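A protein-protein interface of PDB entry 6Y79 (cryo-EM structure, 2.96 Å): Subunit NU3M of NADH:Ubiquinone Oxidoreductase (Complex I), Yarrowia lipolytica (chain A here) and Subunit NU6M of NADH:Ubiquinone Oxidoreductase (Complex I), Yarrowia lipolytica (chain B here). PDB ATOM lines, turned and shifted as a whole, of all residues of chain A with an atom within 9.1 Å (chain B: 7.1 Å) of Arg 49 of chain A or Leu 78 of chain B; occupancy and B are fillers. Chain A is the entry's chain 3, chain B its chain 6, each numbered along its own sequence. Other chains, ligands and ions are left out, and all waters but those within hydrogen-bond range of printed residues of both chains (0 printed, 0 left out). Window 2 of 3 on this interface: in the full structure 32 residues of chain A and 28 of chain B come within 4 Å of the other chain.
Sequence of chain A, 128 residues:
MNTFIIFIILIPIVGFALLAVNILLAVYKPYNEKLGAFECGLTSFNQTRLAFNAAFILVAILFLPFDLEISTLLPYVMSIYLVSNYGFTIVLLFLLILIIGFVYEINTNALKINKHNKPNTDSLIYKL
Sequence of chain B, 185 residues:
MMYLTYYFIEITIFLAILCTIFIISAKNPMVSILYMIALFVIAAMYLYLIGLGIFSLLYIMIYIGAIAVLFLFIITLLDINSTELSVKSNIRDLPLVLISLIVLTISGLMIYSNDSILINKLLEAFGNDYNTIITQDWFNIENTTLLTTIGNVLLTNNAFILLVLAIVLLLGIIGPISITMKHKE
The backbone carbonyl oxygen (O) of Thr 76 of chain B sits at hydrogen-bond distance from the guanidinium group (NH1) of Arg 49 of chain A, 2.8 Å away. The guanidinium group of Arg 49 of chain A sits at hydrogen-bond distance from the backbone carbonyl oxygen of Leu 78 of chain B (3.4 Å).
Leu 77 of chain B touches Arg 49 of chain A (CA to NH1, 3.8 Å). Leu 77 of chain B touches Phe 52 of chain A. Phe 73 of chain B touches Phe 56 of chain A (CZ to O, 3.2 Å). Ile 57 of chain A touches Phe 73 of chain B (CD1 to CE2, 3.6 Å). CD1 of Ile 74 of chain B touches CD1 of Ile 57 of chain A, at 3.6 Å. CD1 of Ile 57 of chain A touches CD1 of Leu 77 of chain B, 3.8 Å away.
Arg 49 of chain A touches three residues of chain B. Of chain A, only Arg 49 comes within 4 Å of Leu 78 of chain B. Of the printed residues of chain A, Thr 76 of chain B touches Arg 49. Of the printed residues of chain A, Phe 73 of chain B touches Phe 56 and Ile 57. The nearest residue of chain B that does not touch Arg 49 of chain A is Asp 79 of chain B (4.1 Å). The nearest residue of chain A that does not touch Leu 78 of chain B is Phe 52 of chain A (4.4 Å).
Hydrophobic or aromatic side chains of chain A within 4 Å of the printed part of chain B: Phe 52 and Ile 57.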
ATOM      1  N   THR A  48      -9.188   5.664  22.183  1.00  0.00           N
ATOM      2  CA  THR A  48     -10.568   5.446  21.782  1.00  0.00           C
ATOM      3  C   THR A  48     -11.044   6.613  20.925  1.00  0.00           C
ATOM      4  O   THR A  48     -11.173   6.509  19.701  1.00  0.00           O
ATOM      5  CB  THR A  48     -11.503   5.300  23.009  1.00  0.00           C
ATOM      6  OG1 THR A  48     -11.035   4.237  23.846  1.00  0.00           O
ATOM      7  CG2 THR A  48     -12.934   4.998  22.576  1.00  0.00           C
ATOM      8  N   ARG A  49     -11.284   7.725  21.615  1.00  0.00           N
ATOM      9  CA  ARG A  49     -11.863   8.965  21.124  1.00  0.00           C
ATOM     10  C   ARG A  49     -11.814   9.931  22.292  1.00  0.00           C
ATOM     11  O   ARG A  49     -11.925   9.510  23.449  1.00  0.00           O
ATOM     12  CB  ARG A  49     -13.310   8.764  20.645  1.00  0.00           C
ATOM     13  CG  ARG A  49     -13.938   9.950  19.955  1.00  0.00           C
ATOM     14  CD  ARG A  49     -13.101  10.410  18.782  1.00  0.00           C
ATOM     15  NE  ARG A  49     -13.366   9.629  17.580  1.00  0.00           N
ATOM     16  CZ  ARG A  49     -13.046  10.025  16.354  1.00  0.00           C
ATOM     17  NH1 ARG A  49     -12.451  11.192  16.168  1.00  0.00           N
ATOM     18  NH2 ARG A  49     -13.319   9.256  15.312  1.00  0.00           N
ATOM     19  N   LEU A  50     -11.632  11.215  21.996  1.00  0.00           N
ATOM     20  CA  LEU A  50     -11.641  12.239  23.026  1.00  0.00           C
ATOM     21  C   LEU A  50     -12.932  13.035  22.959  1.00  0.00           C
ATOM     22  O   LEU A  50     -13.653  13.008  21.960  1.00  0.00           O
ATOM     23  CB  LEU A  50     -10.424  13.176  22.909  1.00  0.00           C
ATOM     24  CG  LEU A  50     -10.103  13.985  21.647  1.00  0.00           C
ATOM     25  CD1 LEU A  50     -10.762  15.367  21.599  1.00  0.00           C
ATOM     26  CD2 LEU A  50      -8.599  14.109  21.508  1.00  0.00           C
ATOM     27  N   ALA A  51     -13.215  13.736  24.046  1.00  0.00           N
ATOM     28  CA  ALA A  51     -14.327  14.661  24.108  1.00  0.00           C
ATOM     29  C   ALA A  51     -13.836  16.079  23.863  1.00  0.00           C
ATOM     30  O   ALA A  51     -12.682  16.417  24.133  1.00  0.00           O
ATOM     31  CB  ALA A  51     -15.024  14.564  25.460  1.00  0.00           C
ATOM     32  N   PHE A  52     -14.740  16.910  23.363  1.00  0.00           N
ATOM     33  CA  PHE A  52     -14.447  18.235  22.849  1.00  0.00           C
ATOM     34  C   PHE A  52     -15.500  19.189  23.382  1.00  0.00           C
ATOM     35  O   PHE A  52     -16.598  18.770  23.739  1.00  0.00           O
ATOM     36  CB  PHE A  52     -14.445  18.246  21.311  1.00  0.00           C
ATOM     37  CG  PHE A  52     -15.667  17.621  20.703  1.00  0.00           C
ATOM     38  CD1 PHE A  52     -15.714  16.259  20.438  1.00  0.00           C
ATOM     39  CD2 PHE A  52     -16.776  18.396  20.392  1.00  0.00           C
ATOM     40  CE1 PHE A  52     -16.840  15.689  19.903  1.00  0.00           C
ATOM     41  CE2 PHE A  52     -17.900  17.823  19.851  1.00  0.00           C
ATOM     42  CZ  PHE A  52     -17.926  16.471  19.592  1.00  0.00           C
ATOM     43  N   PHE A  56     -16.355  24.244  19.611  1.00  0.00           N
ATOM     44  CA  PHE A  56     -15.649  23.703  18.449  1.00  0.00           C
ATOM     45  C   PHE A  56     -16.603  23.300  17.356  1.00  0.00           C
ATOM     46  O   PHE A  56     -16.365  23.551  16.173  1.00  0.00           O
ATOM     47  CB  PHE A  56     -14.869  22.454  18.811  1.00  0.00           C
ATOM     48  CG  PHE A  56     -13.797  22.683  19.742  1.00  0.00           C
ATOM     49  CD1 PHE A  56     -12.596  23.164  19.300  1.00  0.00           C
ATOM     50  CD2 PHE A  56     -13.980  22.415  21.066  1.00  0.00           C
ATOM     51  CE1 PHE A  56     -11.574  23.376  20.168  1.00  0.00           C
ATOM     52  CE2 PHE A  56     -12.972  22.615  21.955  1.00  0.00           C
ATOM     53  CZ  PHE A  56     -11.791  23.086  21.485  1.00  0.00           C
ATOM     54  N   ILE A  57     -17.633  22.560  17.728  1.00  0.00           N
ATOM     55  CA  ILE A  57     -18.566  22.117  16.720  1.00  0.00           C
ATOM     56  C   ILE A  57     -19.472  23.275  16.357  1.00  0.00           C
ATOM     57  O   ILE A  57     -19.911  23.397  15.206  1.00  0.00           O
ATOM     58  CB  ILE A  57     -19.304  20.865  17.231  1.00  0.00           C
ATOM     59  CG1 ILE A  57     -19.981  20.168  16.079  1.00  0.00           C
ATOM     60  CG2 ILE A  57     -20.245  21.151  18.400  1.00  0.00           C
ATOM     61  CD1 ILE A  57     -18.986  19.456  15.259  1.00  0.00           C
ATOM     62  N   ILE A  61     -20.722  24.832  12.686  1.00  0.00           N
ATOM     63  CA  ILE A  61     -22.138  24.716  12.354  1.00  0.00           C
ATOM     64  C   ILE A  61     -22.740  26.094  12.115  1.00  0.00           C
ATOM     65  O   ILE A  61     -23.369  26.330  11.079  1.00  0.00           O
ATOM     66  CB  ILE A  61     -22.917  23.928  13.419  1.00  0.00           C
ATOM     67  CG1 ILE A  61     -22.471  22.472  13.445  1.00  0.00           C
ATOM     68  CG2 ILE A  61     -24.356  23.899  13.048  1.00  0.00           C
ATOM     69  CD1 ILE A  61     -23.092  21.664  14.560  1.00  0.00           C
ATOM     70  N   PHE B  73     -15.891  17.923   8.576  1.00  0.00           N
ATOM     71  CA  PHE B  73     -15.679  18.374   9.941  1.00  0.00           C
ATOM     72  C   PHE B  73     -16.481  17.550  10.946  1.00  0.00           C
ATOM     73  O   PHE B  73     -16.035  17.360  12.081  1.00  0.00           O
ATOM     74  CB  PHE B  73     -16.060  19.857   9.986  1.00  0.00           C
ATOM     75  CG  PHE B  73     -15.758  20.547  11.267  1.00  0.00           C
ATOM     76  CD1 PHE B  73     -14.543  21.171  11.459  1.00  0.00           C
ATOM     77  CD2 PHE B  73     -16.712  20.623  12.264  1.00  0.00           C
ATOM     78  CE1 PHE B  73     -14.275  21.830  12.637  1.00  0.00           C
ATOM     79  CE2 PHE B  73     -16.443  21.267  13.444  1.00  0.00           C
ATOM     80  CZ  PHE B  73     -15.226  21.876  13.632  1.00  0.00           C
ATOM     81  N   ILE B  74     -17.664  17.070  10.555  1.00  0.00           N
ATOM     82  CA  ILE B  74     -18.448  16.198  11.432  1.00  0.00           C
ATOM     83  C   ILE B  74     -17.809  14.818  11.528  1.00  0.00           C
ATOM     84  O   ILE B  74     -17.679  14.256  12.621  1.00  0.00           O
ATOM     85  CB  ILE B  74     -19.908  16.110  10.944  1.00  0.00           C
ATOM     86  CG1 ILE B  74     -20.641  17.424  11.179  1.00  0.00           C
ATOM     87  CG2 ILE B  74     -20.671  15.004  11.653  1.00  0.00           C
ATOM     88  CD1 ILE B  74     -20.815  17.794  12.597  1.00  0.00           C
ATOM     89  N   ILE B  75     -17.395  14.256  10.387  1.00  0.00           N
ATOM     90  CA  ILE B  75     -16.853  12.891  10.369  1.00  0.00           C
ATOM     91  C   ILE B  75     -15.546  12.787  11.140  1.00  0.00           C
ATOM     92  O   ILE B  75     -15.257  11.745  11.746  1.00  0.00           O
ATOM     93  CB  ILE B  75     -16.675  12.425   8.916  1.00  0.00           C
ATOM     94  CG1 ILE B  75     -18.010  12.426   8.229  1.00  0.00           C
ATOM     95  CG2 ILE B  75     -16.140  11.006   8.804  1.00  0.00           C
ATOM     96  CD1 ILE B  75     -17.824  12.447   6.811  1.00  0.00           C
ATOM     97  N   THR B  76     -14.754  13.859  11.161  1.00  0.00           N
ATOM     98  CA  THR B  76     -13.494  13.844  11.895  1.00  0.00           C
ATOM     99  C   THR B  76     -13.645  13.601  13.396  1.00  0.00           C
ATOM    100  O   THR B  76     -13.123  12.605  13.906  1.00  0.00           O
ATOM    101  CB  THR B  76     -12.739  15.146  11.662  1.00  0.00           C
ATOM    102  OG1 THR B  76     -12.588  15.359  10.258  1.00  0.00           O
ATOM    103  CG2 THR B  76     -11.386  15.070  12.289  1.00  0.00           C
ATOM    104  N   LEU B  77     -14.365  14.458  14.116  1.00  0.00           N
ATOM    105  CA  LEU B  77     -14.380  14.367  15.569  1.00  0.00           C
ATOM    106  C   LEU B  77     -15.615  13.671  16.135  1.00  0.00           C
ATOM    107  O   LEU B  77     -15.940  13.868  17.308  1.00  0.00           O
ATOM    108  CB  LEU B  77     -14.188  15.754  16.193  1.00  0.00           C
ATOM    109  CG  LEU B  77     -14.924  17.046  15.819  1.00  0.00           C
ATOM    110  CD1 LEU B  77     -16.250  17.149  16.462  1.00  0.00           C
ATOM    111  CD2 LEU B  77     -14.125  18.186  16.338  1.00  0.00           C
ATOM    112  N   LEU B  78     -16.275  12.823  15.355  1.00  0.00           N
ATOM    113  CA  LEU B  78     -17.352  11.985  15.862  1.00  0.00           C
ATOM    114  C   LEU B  78     -17.108  10.545  15.434  1.00  0.00           C
ATOM    115  O   LEU B  78     -16.474  10.284  14.411  1.00  0.00           O
ATOM    116  CB  LEU B  78     -18.730  12.451  15.377  1.00  0.00           C
ATOM    117  CG  LEU B  78     -19.381  13.618  16.123  1.00  0.00           C
ATOM    118  CD1 LEU B  78     -18.953  14.926  15.577  1.00  0.00           C
ATOM    119  CD2 LEU B  78     -20.849  13.538  16.018  1.00  0.00           C
ATOM    120  N   ASP B  79     -17.622   9.602  16.222  1.00  0.00           N
ATOM    121  CA  ASP B  79     -17.393   8.185  15.964  1.00  0.00           C
ATOM    122  C   ASP B  79     -18.610   7.569  15.294  1.00  0.00           C
ATOM    123  O   ASP B  79     -19.724   7.636  15.822  1.00  0.00           O
ATOM    124  CB  ASP B  79     -17.056   7.419  17.239  1.00  0.00           C
ATOM    125  CG  ASP B  79     -16.456   6.058  16.939  1.00  0.00           C
ATOM    126  OD1 ASP B  79     -15.607   5.973  16.026  1.00  0.00           O
ATOM    127  OD2 ASP B  79     -16.840   5.071  17.599  1.00  0.00           O
ATOM    128  N   ILE B  80     -18.378   6.944  14.145  1.00  0.00           N
ATOM    129  CA  ILE B  80     -19.417   6.398  13.285  1.00  0.00           C
ATOM    130  C   ILE B  80     -18.982   4.991  12.913  1.00  0.00           C
ATOM    131  O   ILE B  80     -17.938   4.811  12.276  1.00  0.00           O
ATOM    132  CB  ILE B  80     -19.631   7.258  12.032  1.00  0.00           C
ATOM    133  CG1 ILE B  80     -20.284   8.584  12.403  1.00  0.00           C
ATOM    134  CG2 ILE B  80     -20.478   6.529  11.004  1.00  0.00           C
ATOM    135  CD1 ILE B  80     -19.756   9.740  11.620  1.00  0.00           C
